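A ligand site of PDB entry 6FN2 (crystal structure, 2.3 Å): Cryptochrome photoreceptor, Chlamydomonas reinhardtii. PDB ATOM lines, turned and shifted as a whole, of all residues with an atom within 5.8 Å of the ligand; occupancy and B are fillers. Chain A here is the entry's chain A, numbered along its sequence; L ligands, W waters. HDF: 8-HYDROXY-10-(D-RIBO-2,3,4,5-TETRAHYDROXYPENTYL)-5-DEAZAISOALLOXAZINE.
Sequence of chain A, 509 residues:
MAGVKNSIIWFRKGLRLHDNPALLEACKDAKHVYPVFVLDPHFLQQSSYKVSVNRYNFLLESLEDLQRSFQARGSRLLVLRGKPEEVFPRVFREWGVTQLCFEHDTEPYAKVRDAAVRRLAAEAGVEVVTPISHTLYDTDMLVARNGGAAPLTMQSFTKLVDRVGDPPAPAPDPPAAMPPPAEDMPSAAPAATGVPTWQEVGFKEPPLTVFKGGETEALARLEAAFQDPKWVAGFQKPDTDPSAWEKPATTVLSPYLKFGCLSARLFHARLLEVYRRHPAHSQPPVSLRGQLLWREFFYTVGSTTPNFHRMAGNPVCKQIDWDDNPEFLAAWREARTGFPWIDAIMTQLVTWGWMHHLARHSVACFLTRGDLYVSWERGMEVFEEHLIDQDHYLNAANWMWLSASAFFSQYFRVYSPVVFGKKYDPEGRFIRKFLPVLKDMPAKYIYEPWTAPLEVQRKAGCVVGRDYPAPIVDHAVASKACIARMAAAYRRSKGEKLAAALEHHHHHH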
ATOM      1  N   TRP A  10       0.269  -9.245  27.199  1.00  0.00           N
ATOM      2  CA  TRP A  10      -1.142  -9.071  26.939  1.00  0.00           C
ATOM      3  C   TRP A  10      -1.315  -8.514  25.514  1.00  0.00           C
ATOM      4  O   TRP A  10      -0.818  -7.445  25.210  1.00  0.00           O
ATOM      5  CB  TRP A  10      -1.777  -8.192  28.025  1.00  0.00           C
ATOM      6  CG  TRP A  10      -3.261  -7.888  27.857  1.00  0.00           C
ATOM      7  CD1 TRP A  10      -4.174  -8.651  27.220  1.00  0.00           C
ATOM      8  CD2 TRP A  10      -3.956  -6.744  28.354  1.00  0.00           C
ATOM      9  NE1 TRP A  10      -5.412  -8.065  27.290  1.00  0.00           N
ATOM     10  CE2 TRP A  10      -5.306  -6.877  27.970  1.00  0.00           C
ATOM     11  CE3 TRP A  10      -3.582  -5.608  29.077  1.00  0.00           C
ATOM     12  CZ2 TRP A  10      -6.278  -5.931  28.289  1.00  0.00           C
ATOM     13  CZ3 TRP A  10      -4.545  -4.659  29.395  1.00  0.00           C
ATOM     14  CH2 TRP A  10      -5.892  -4.841  29.002  1.00  0.00           C
ATOM     15  N   PHE A  11      -1.978  -9.290  24.663  1.00  0.00           N
ATOM     16  CA  PHE A  11      -2.306  -8.945  23.290  1.00  0.00           C
ATOM     17  C   PHE A  11      -3.711  -8.347  23.237  1.00  0.00           C
ATOM     18  O   PHE A  11      -4.641  -8.860  23.863  1.00  0.00           O
ATOM     19  CB  PHE A  11      -2.290 -10.204  22.399  1.00  0.00           C
ATOM     20  CG  PHE A  11      -0.925 -10.784  22.214  1.00  0.00           C
ATOM     21  CD1 PHE A  11      -0.416 -11.711  23.116  1.00  0.00           C
ATOM     22  CD2 PHE A  11      -0.133 -10.395  21.142  1.00  0.00           C
ATOM     23  CE1 PHE A  11       0.864 -12.244  22.949  1.00  0.00           C
ATOM     24  CE2 PHE A  11       1.125 -10.930  20.957  1.00  0.00           C
ATOM     25  CZ  PHE A  11       1.637 -11.861  21.878  1.00  0.00           C
ATOM     26  N   ARG A  12      -3.869  -7.270  22.486  1.00  0.00           N
ATOM     27  CA  ARG A  12      -5.185  -6.655  22.263  1.00  0.00           C
ATOM     28  C   ARG A  12      -5.258  -6.352  20.772  1.00  0.00           C
ATOM     29  O   ARG A  12      -6.047  -6.955  20.037  1.00  0.00           O
ATOM     30  CB  ARG A  12      -5.402  -5.421  23.162  1.00  0.00           C
ATOM     31  CG  ARG A  12      -5.030  -5.607  24.640  1.00  0.00           C
ATOM     32  CD  ARG A  12      -3.563  -5.283  24.922  1.00  0.00           C
ATOM     33  NE  ARG A  12      -3.276  -3.876  24.640  1.00  0.00           N
ATOM     34  CZ  ARG A  12      -3.574  -2.855  25.438  1.00  0.00           C
ATOM     35  NH1 ARG A  12      -3.292  -1.596  25.049  1.00  0.00           N
ATOM     36  NH2 ARG A  12      -4.150  -3.062  26.631  1.00  0.00           N
ATOM     37  N   LYS A  13      -4.406  -5.423  20.331  1.00  0.00           N
ATOM     38  CA  LYS A  13      -3.927  -5.384  18.956  1.00  0.00           C
ATOM     39  C   LYS A  13      -2.532  -6.013  19.045  1.00  0.00           C
ATOM     40  O   LYS A  13      -2.232  -6.745  20.005  1.00  0.00           O
ATOM     41  CB  LYS A  13      -3.876  -3.932  18.453  1.00  0.00           C
ATOM     42  CG  LYS A  13      -5.158  -3.134  18.617  1.00  0.00           C
ATOM     43  CD  LYS A  13      -4.957  -1.748  18.024  1.00  0.00           C
ATOM     44  CE  LYS A  13      -6.200  -0.879  18.154  1.00  0.00           C
ATOM     45  NZ  LYS A  13      -6.011   0.529  17.638  1.00  0.00           N
ATOM     46  N   PHE A  37      -4.774 -13.070  25.753  1.00  0.00           N
ATOM     47  CA  PHE A  37      -5.745 -12.231  25.072  1.00  0.00           C
ATOM     48  C   PHE A  37      -7.033 -12.371  25.865  1.00  0.00           C
ATOM     49  O   PHE A  37      -7.443 -13.483  26.193  1.00  0.00           O
ATOM     50  CB  PHE A  37      -5.948 -12.697  23.642  1.00  0.00           C
ATOM     51  CG  PHE A  37      -6.862 -11.828  22.836  1.00  0.00           C
ATOM     52  CD1 PHE A  37      -8.238 -12.046  22.829  1.00  0.00           C
ATOM     53  CD2 PHE A  37      -6.347 -10.819  22.029  1.00  0.00           C
ATOM     54  CE1 PHE A  37      -9.077 -11.249  22.064  1.00  0.00           C
ATOM     55  CE2 PHE A  37      -7.189 -10.010  21.256  1.00  0.00           C
ATOM     56  CZ  PHE A  37      -8.553 -10.229  21.267  1.00  0.00           C
ATOM     57  N   VAL A  38      -7.649 -11.245  26.197  1.00  0.00           N
ATOM     58  CA  VAL A  38      -8.869 -11.258  26.985  1.00  0.00           C
ATOM     59  C   VAL A  38     -10.021 -11.118  26.015  1.00  0.00           C
ATOM     60  O   VAL A  38     -10.191 -10.080  25.381  1.00  0.00           O
ATOM     61  CB  VAL A  38      -8.843 -10.143  28.060  1.00  0.00           C
ATOM     62  CG1 VAL A  38     -10.146 -10.091  28.828  1.00  0.00           C
ATOM     63  CG2 VAL A  38      -7.683 -10.385  29.021  1.00  0.00           C
ATOM     64  N   LEU A  39     -10.796 -12.188  25.860  1.00  0.00           N
ATOM     65  CA  LEU A  39     -11.993 -12.192  25.012  1.00  0.00           C
ATOM     66  C   LEU A  39     -13.072 -11.432  25.779  1.00  0.00           C
ATOM     67  O   LEU A  39     -13.735 -11.982  26.675  1.00  0.00           O
ATOM     68  CB  LEU A  39     -12.411 -13.611  24.622  1.00  0.00           C
ATOM     69  CG  LEU A  39     -13.112 -13.742  23.267  1.00  0.00           C
ATOM     70  CD1 LEU A  39     -12.124 -13.507  22.125  1.00  0.00           C
ATOM     71  CD2 LEU A  39     -13.736 -15.119  23.111  1.00  0.00           C
ATOM     72  N   ASP A  40     -13.211 -10.157  25.419  1.00  0.00           N
ATOM     73  CA  ASP A  40     -13.826  -9.146  26.251  1.00  0.00           C
ATOM     74  C   ASP A  40     -15.299  -8.940  25.809  1.00  0.00           C
ATOM     75  O   ASP A  40     -15.547  -8.654  24.621  1.00  0.00           O
ATOM     76  CB  ASP A  40     -12.991  -7.879  26.098  1.00  0.00           C
ATOM     77  CG  ASP A  40     -13.482  -6.685  26.928  1.00  0.00           C
ATOM     78  OD1 ASP A  40     -14.625  -6.668  27.416  1.00  0.00           O
ATOM     79  OD2 ASP A  40     -12.661  -5.739  27.076  1.00  0.00           O
ATOM     80  N   PRO A  41     -16.259  -9.063  26.753  1.00  0.00           N
ATOM     81  CA  PRO A  41     -17.685  -8.893  26.391  1.00  0.00           C
ATOM     82  C   PRO A  41     -18.052  -7.520  25.819  1.00  0.00           C
ATOM     83  O   PRO A  41     -19.052  -7.420  25.090  1.00  0.00           O
ATOM     84  CB  PRO A  41     -18.436  -9.155  27.717  1.00  0.00           C
ATOM     85  CG  PRO A  41     -17.435  -8.891  28.786  1.00  0.00           C
ATOM     86  CD  PRO A  41     -16.109  -9.315  28.204  1.00  0.00           C
ATOM     87  N   PHE A  43     -16.941  -6.126  23.245  1.00  0.00           N
ATOM     88  CA  PHE A  43     -16.955  -6.172  21.777  1.00  0.00           C
ATOM     89  C   PHE A  43     -18.054  -7.103  21.244  1.00  0.00           C
ATOM     90  O   PHE A  43     -18.221  -7.212  20.027  1.00  0.00           O
ATOM     91  CB  PHE A  43     -15.571  -6.601  21.249  1.00  0.00           C
ATOM     92  CG  PHE A  43     -14.439  -5.752  21.765  1.00  0.00           C
ATOM     93  CD1 PHE A  43     -13.821  -6.048  22.981  1.00  0.00           C
ATOM     94  CD2 PHE A  43     -14.001  -4.637  21.056  1.00  0.00           C
ATOM     95  CE1 PHE A  43     -12.807  -5.268  23.467  1.00  0.00           C
ATOM     96  CE2 PHE A  43     -12.976  -3.855  21.551  1.00  0.00           C
ATOM     97  CZ  PHE A  43     -12.374  -4.173  22.745  1.00  0.00           C
ATOM     98  N   TYR A  49     -21.101  -0.716  20.037  1.00  0.00           N
ATOM     99  CA  TYR A  49     -20.052  -1.409  19.264  1.00  0.00           C
ATOM    100  C   TYR A  49     -20.671  -2.519  18.400  1.00  0.00           C
ATOM    101  O   TYR A  49     -21.377  -3.401  18.904  1.00  0.00           O
ATOM    102  CB  TYR A  49     -18.887  -1.945  20.121  1.00  0.00           C
ATOM    103  CG  TYR A  49     -17.683  -2.323  19.265  1.00  0.00           C
ATOM    104  CD1 TYR A  49     -16.883  -1.349  18.695  1.00  0.00           C
ATOM    105  CD2 TYR A  49     -17.376  -3.665  19.001  1.00  0.00           C
ATOM    106  CE1 TYR A  49     -15.803  -1.682  17.912  1.00  0.00           C
ATOM    107  CE2 TYR A  49     -16.294  -4.005  18.206  1.00  0.00           C
ATOM    108  CZ  TYR A  49     -15.511  -2.999  17.665  1.00  0.00           C
ATOM    109  OH  TYR A  49     -14.438  -3.311  16.875  1.00  0.00           O
ATOM    110  N   VAL A  51     -20.083  -5.495  15.187  1.00  0.00           N
ATOM    111  CA  VAL A  51     -19.084  -6.375  14.591  1.00  0.00           C
ATOM    112  C   VAL A  51     -19.732  -7.540  13.843  1.00  0.00           C
ATOM    113  O   VAL A  51     -20.498  -8.306  14.425  1.00  0.00           O
ATOM    114  CB  VAL A  51     -18.035  -6.866  15.633  1.00  0.00           C
ATOM    115  CG1 VAL A  51     -18.665  -7.749  16.700  1.00  0.00           C
ATOM    116  CG2 VAL A  51     -16.887  -7.593  14.955  1.00  0.00           C
ATOM    117  N   ARG A  55     -15.413  -9.809  10.542  1.00  0.00           N
ATOM    118  CA  ARG A  55     -14.321  -9.237  11.319  1.00  0.00           C
ATOM    119  C   ARG A  55     -13.975 -10.118  12.493  1.00  0.00           C
ATOM    120  O   ARG A  55     -12.809 -10.393  12.711  1.00  0.00           O
ATOM    121  CB  ARG A  55     -14.558  -7.798  11.817  1.00  0.00           C
ATOM    122  CG  ARG A  55     -13.295  -7.230  12.482  1.00  0.00           C
ATOM    123  CD  ARG A  55     -13.131  -5.708  12.449  1.00  0.00           C
ATOM    124  NE  ARG A  55     -13.984  -5.070  13.435  1.00  0.00           N
ATOM    125  CZ  ARG A  55     -15.246  -4.671  13.259  1.00  0.00           C
ATOM    126  NH1 ARG A  55     -15.881  -4.812  12.089  1.00  0.00           N
ATOM    127  NH2 ARG A  55     -15.877  -4.108  14.289  1.00  0.00           N
ATOM    128  N   TYR A  56     -14.980 -10.561  13.241  1.00  0.00           N
ATOM    129  CA  TYR A  56     -14.727 -11.373  14.417  1.00  0.00           C
ATOM    130  C   TYR A  56     -14.011 -12.702  14.079  1.00  0.00           C
ATOM    131  O   TYR A  56     -13.097 -13.119  14.792  1.00  0.00           O
ATOM    132  CB  TYR A  56     -16.023 -11.630  15.211  1.00  0.00           C
ATOM    133  CG  TYR A  56     -15.725 -11.813  16.678  1.00  0.00           C
ATOM    134  CD1 TYR A  56     -15.280 -13.039  17.156  1.00  0.00           C
ATOM    135  CD2 TYR A  56     -15.849 -10.755  17.576  1.00  0.00           C
ATOM    136  CE1 TYR A  56     -14.994 -13.209  18.494  1.00  0.00           C
ATOM    137  CE2 TYR A  56     -15.543 -10.921  18.922  1.00  0.00           C
ATOM    138  CZ  TYR A  56     -15.111 -12.144  19.371  1.00  0.00           C
ATOM    139  OH  TYR A  56     -14.805 -12.349  20.700  1.00  0.00           O
ATOM    140  N   LEU A  59     -10.326 -11.880  13.425  1.00  0.00           N
ATOM    141  CA  LEU A  59      -9.706 -11.905  14.761  1.00  0.00           C
ATOM    142  C   LEU A  59      -9.372 -13.319  15.289  1.00  0.00           C
ATOM    143  O   LEU A  59      -8.249 -13.589  15.677  1.00  0.00           O
ATOM    144  CB  LEU A  59     -10.586 -11.172  15.767  1.00  0.00           C
ATOM    145  CG  LEU A  59     -10.199 -11.227  17.247  1.00  0.00           C
ATOM    146  CD1 LEU A  59      -8.811 -10.645  17.451  1.00  0.00           C
ATOM    147  CD2 LEU A  59     -11.215 -10.460  18.060  1.00  0.00           C
ATOM    148  N   ASP A 105      -2.155   1.418  23.211  1.00  0.00           N
ATOM    149  CA  ASP A 105      -3.167   1.864  22.228  1.00  0.00           C
ATOM    150  C   ASP A 105      -3.791   3.163  22.734  1.00  0.00           C
ATOM    151  O   ASP A 105      -3.736   3.478  23.929  1.00  0.00           O
ATOM    152  CB  ASP A 105      -4.244   0.802  21.945  1.00  0.00           C
ATOM    153  CG  ASP A 105      -5.133   1.171  20.731  1.00  0.00           C
ATOM    154  OD1 ASP A 105      -4.621   1.714  19.718  1.00  0.00           O
ATOM    155  OD2 ASP A 105      -6.351   0.929  20.793  1.00  0.00           O
ATOM    156  N   GLU A 107      -7.037   4.452  21.560  1.00  0.00           N
ATOM    157  CA  GLU A 107      -8.490   4.547  21.423  1.00  0.00           C
ATOM    158  C   GLU A 107      -9.155   4.857  22.758  1.00  0.00           C
ATOM    159  O   GLU A 107      -8.549   4.602  23.810  1.00  0.00           O
ATOM    160  CB  GLU A 107      -9.073   3.266  20.861  1.00  0.00           C
ATOM    161  CG  GLU A 107      -8.592   2.962  19.455  1.00  0.00           C
ATOM    162  CD  GLU A 107      -9.304   1.794  18.846  1.00  0.00           C
ATOM    163  OE1 GLU A 107     -10.324   1.330  19.419  1.00  0.00           O
ATOM    164  OE2 GLU A 107      -8.848   1.327  17.782  1.00  0.00           O
ATOM    165  N   PRO A 108     -10.376   5.436  22.733  1.00  0.00           N
ATOM    166  CA  PRO A 108     -11.103   5.759  23.976  1.00  0.00           C
ATOM    167  C   PRO A 108     -11.282   4.596  24.953  1.00  0.00           C
ATOM    168  O   PRO A 108     -11.020   4.774  26.162  1.00  0.00           O
ATOM    169  CB  PRO A 108     -12.460   6.241  23.478  1.00  0.00           C
ATOM    170  CG  PRO A 108     -12.189   6.789  22.125  1.00  0.00           C
ATOM    171  CD  PRO A 108     -11.140   5.886  21.550  1.00  0.00           C
ATOM    172  N   TYR A 109     -11.740   3.440  24.461  1.00  0.00           N
ATOM    173  CA  TYR A 109     -11.900   2.256  25.310  1.00  0.00           C
ATOM    174  C   TYR A 109     -10.549   1.811  25.877  1.00  0.00           C
ATOM    175  O   TYR A 109     -10.412   1.587  27.078  1.00  0.00           O
ATOM    176  CB  TYR A 109     -12.558   1.089  24.563  1.00  0.00           C
ATOM    177  CG  TYR A 109     -12.726  -0.135  25.436  1.00  0.00           C
ATOM    178  CD1 TYR A 109     -13.506  -0.076  26.607  1.00  0.00           C
ATOM    179  CD2 TYR A 109     -12.115  -1.350  25.120  1.00  0.00           C
ATOM    180  CE1 TYR A 109     -13.678  -1.192  27.418  1.00  0.00           C
ATOM    181  CE2 TYR A 109     -12.264  -2.470  25.928  1.00  0.00           C
ATOM    182  CZ  TYR A 109     -13.055  -2.378  27.076  1.00  0.00           C
ATOM    183  OH  TYR A 109     -13.212  -3.471  27.900  1.00  0.00           O
ATOM    184  N   ALA A 110      -9.553   1.709  24.991  1.00  0.00           N
ATOM    185  CA  ALA A 110      -8.204   1.343  25.377  1.00  0.00           C
ATOM    186  C   ALA A 110      -7.670   2.197  26.553  1.00  0.00           C
ATOM    187  O   ALA A 110      -7.140   1.645  27.509  1.00  0.00           O
ATOM    188  CB  ALA A 110      -7.277   1.423  24.194  1.00  0.00           C
ATOM    189  N   ARG A 113      -9.790   1.270  29.813  1.00  0.00           N
ATOM    190  CA  ARG A 113      -9.349  -0.079  30.167  1.00  0.00           C
ATOM    191  C   ARG A 113      -7.922  -0.072  30.693  1.00  0.00           C
ATOM    192  O   ARG A 113      -7.666  -0.629  31.771  1.00  0.00           O
ATOM    193  CB  ARG A 113      -9.452  -0.994  28.943  1.00  0.00           C
ATOM    194  CG  ARG A 113      -9.001  -2.446  29.144  1.00  0.00           C
ATOM    195  CD  ARG A 113      -8.919  -3.159  27.802  1.00  0.00           C
ATOM    196  NE  ARG A 113      -7.964  -2.505  26.892  1.00  0.00           N
ATOM    197  CZ  ARG A 113      -7.893  -2.706  25.570  1.00  0.00           C
ATOM    198  NH1 ARG A 113      -8.702  -3.572  24.955  1.00  0.00           N
ATOM    199  NH2 ARG A 113      -6.988  -2.052  24.850  1.00  0.00           N
ATOM    200  N   LYS A 258      -4.620  -3.070  11.128  1.00  0.00           N
ATOM    201  CA  LYS A 258      -5.628  -2.796  12.138  1.00  0.00           C
ATOM    202  C   LYS A 258      -5.482  -3.693  13.382  1.00  0.00           C
ATOM    203  O   LYS A 258      -5.467  -3.177  14.525  1.00  0.00           O
ATOM    204  CB  LYS A 258      -7.025  -2.925  11.525  1.00  0.00           C
ATOM    205  CG  LYS A 258      -8.140  -2.611  12.503  1.00  0.00           C
ATOM    206  CD  LYS A 258      -8.717  -3.870  13.161  1.00  0.00           C
ATOM    207  CE  LYS A 258      -8.995  -3.678  14.657  1.00  0.00           C
ATOM    208  NZ  LYS A 258     -10.172  -2.827  14.910  1.00  0.00           N
ATOM    209  N   PHE A 259      -5.337  -5.004  13.163  1.00  0.00           N
ATOM    210  CA  PHE A 259      -5.119  -5.966  14.254  1.00  0.00           C
ATOM    211  C   PHE A 259      -3.657  -6.095  14.721  1.00  0.00           C
ATOM    212  O   PHE A 259      -3.367  -6.661  15.784  1.00  0.00           O
ATOM    213  CB  PHE A 259      -5.696  -7.337  13.880  1.00  0.00           C
ATOM    214  CG  PHE A 259      -7.181  -7.401  14.004  1.00  0.00           C
ATOM    215  CD1 PHE A 259      -7.773  -7.395  15.268  1.00  0.00           C
ATOM    216  CD2 PHE A 259      -8.002  -7.392  12.882  1.00  0.00           C
ATOM    217  CE1 PHE A 259      -9.154  -7.423  15.407  1.00  0.00           C
ATOM    218  CE2 PHE A 259      -9.384  -7.419  13.011  1.00  0.00           C
ATOM    219  CZ  PHE A 259      -9.955  -7.449  14.276  1.00  0.00           C
ATOM    220  N   GLN A 390     -11.933  -2.432  10.099  1.00  0.00           N
ATOM    221  CA  GLN A 390     -12.571  -1.383  10.920  1.00  0.00           C
ATOM    222  C   GLN A 390     -11.590  -0.876  11.963  1.00  0.00           C
ATOM    223  O   GLN A 390     -11.088  -1.652  12.790  1.00  0.00           O
ATOM    224  CB  GLN A 390     -13.885  -1.860  11.574  1.00  0.00           C
ATOM    225  CG  GLN A 390     -14.230  -1.340  12.983  1.00  0.00           C
ATOM    226  CD  GLN A 390     -14.352   0.186  13.065  1.00  0.00           C
ATOM    227  OE1 GLN A 390     -14.596   0.859  12.057  1.00  0.00           O
ATOM    228  NE2 GLN A 390     -14.182   0.721  14.275  1.00  0.00           N
HETATM  229  N1  HDF L   1      -9.463  -6.650  21.875  1.00  0.00           N
HETATM  230  C2  HDF L   1      -9.569  -7.342  23.020  1.00  0.00           C
HETATM  231  O2  HDF L   1      -8.701  -7.135  23.880  1.00  0.00           O
HETATM  232  N3  HDF L   1     -10.550  -8.236  23.226  1.00  0.00           N
HETATM  233  C4  HDF L   1     -11.507  -8.471  22.331  1.00  0.00           C
HETATM  234  O4  HDF L   1     -12.419  -9.303  22.581  1.00  0.00           O
HETATM  235  C4A HDF L   1     -11.479  -7.717  21.041  1.00  0.00           C
HETATM  236  C5  HDF L   1     -12.431  -7.877  20.047  1.00  0.00           C
HETATM  237  C5A HDF L   1     -12.350  -7.141  18.861  1.00  0.00           C
HETATM  238  C6  HDF L   1     -13.311  -7.305  17.876  1.00  0.00           C
HETATM  239  C7  HDF L   1     -13.240  -6.572  16.691  1.00  0.00           C
HETATM  240  C8  HDF L   1     -12.189  -5.662  16.501  1.00  0.00           C
HETATM  241  O8  HDF L   1     -12.073  -4.928  15.372  1.00  0.00           O
HETATM  242  C9  HDF L   1     -11.207  -5.467  17.468  1.00  0.00           C
HETATM  243  C9A HDF L   1     -11.224  -6.168  18.673  1.00  0.00           C
HETATM  244  N10 HDF L   1     -10.259  -5.970  19.704  1.00  0.00           N
HETATM  245  C10 HDF L   1     -10.367  -6.763  20.873  1.00  0.00           C
HETATM  246  C1' HDF L   1      -9.063  -5.124  19.557  1.00  0.00           C
HETATM  247  C2' HDF L   1      -8.817  -3.645  19.794  1.00  0.00           C
HETATM  248  O2' HDF L   1      -9.783  -2.909  19.052  1.00  0.00           O
HETATM  249  C3' HDF L   1      -8.376  -3.312  21.255  1.00  0.00           C
HETATM  250  O3' HDF L   1      -8.932  -4.173  22.267  1.00  0.00           O
HETATM  251  C4' HDF L   1      -8.476  -1.874  21.788  1.00  0.00           C
HETATM  252  O4' HDF L   1      -7.197  -1.273  21.660  1.00  0.00           O
HETATM  253  C5' HDF L   1      -9.557  -0.988  21.240  1.00  0.00           C
HETATM  254  O5' HDF L   1      -9.809   0.117  22.150  1.00  0.00           O
HETATM  255  O   HOH W   1      -9.940  -5.878  26.256  1.00  0.00           O
HETATM  256  O   HOH W   2      -6.975  -8.689  25.034  1.00  0.00           O
HETATM  257  O   HOH W   3     -14.824 -10.186  22.223  1.00  0.00           O
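The side-chain carboxylate (OD2) of Asp 105 sits at hydrogen-bond distance from an oxygen (O4') of the ligand (2.5 Å).
O8 of the ligand is in hydrogen-bond range of NE of Arg 55, 2.7 Å away.
The guanidinium group (NH1) of Arg 113 lies within hydrogen-bond range of an oxygen (O3') of the ligand (2.8 Å).
A nitrogen (N3) of the ligand lies within hydrogen-bond range of the backbone carbonyl oxygen (O) of Val 38 (2.9 Å).
The side-chain amino group of Lys 258 is in hydrogen-bond range of an oxygen (O8) of the ligand (2.9 Å).
O5' of the ligand sits at hydrogen-bond distance from OE1 of Glu 107.
N of Asp 40 lies within hydrogen-bond range of O4 of the ligand.
The side-chain hydroxyl (OH) of Tyr 49 is in hydrogen-bond range of an oxygen (O8) of the ligand (3.2 Å).
The backbone NH (N) of Ala 110 is in hydrogen-bond range of an oxygen (O5') of the ligand.
OD1 of Asp 105 is in salt-bridge range of NZ of Lys 13, at 2.8 Å.
The guanidinium group (NH2) of Arg 55 sits at hydrogen-bond distance from the side-chain hydroxyl (OH) of Tyr 49 (3.1 Å).
NZ of Lys 258 lies within hydrogen-bond range of O of Gln 390.
The side-chain carboxylate (OE2) of Glu 107 is in salt-bridge range of the side-chain amino group (NZ) of Lys 13, 3.0 Å away.
The side-chain carboxylate (OD2) of Asp 40 sits at hydrogen-bond distance from the side-chain hydroxyl (OH) of Tyr 109 (2.5 Å).
Merely in contact with the ligand: Phe 43, Phe 37, Phe 259, Leu 59, Arg 12, Lys 13, Tyr 109 and Leu 39.
Hydrophobic or aromatic side chains that line the ligand: Phe 37, Phe 43, Leu 59, Tyr 109, Ala 110 and Phe 259.
Within 4 Å of the ligand: Arg 12, Lys 13, Phe 37, Val 38, Leu 39, Asp 40, Phe 43, Tyr 49, Arg 55, Leu 59, Asp 105, Glu 107, Tyr 109, Ala 110, Arg 113, Lys 258 and Phe 259.
Water W3 lies within hydrogen-bond range of an oxygen (O4) of the ligand (2.6 Å), the side-chain hydroxyl of Tyr 56 (2.6 Å) and the backbone carbonyl oxygen of Asp 40 (2.9 Å).
Water W2 lies within hydrogen-bond range of an oxygen (O2) of the ligand, the backbone carbonyl oxygen (O) of Phe 11, the indole nitrogen (NE1) of Trp 10 and the backbone NH (N) of Val 38.
Water W1 lies within hydrogen-bond range of the side-chain carboxylate (OD2) of Asp 40 (2.8 Å), the guanidinium group (NH1) of Arg 113 (2.9 Å) and an oxygen (O2) of the ligand (3.0 Å).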
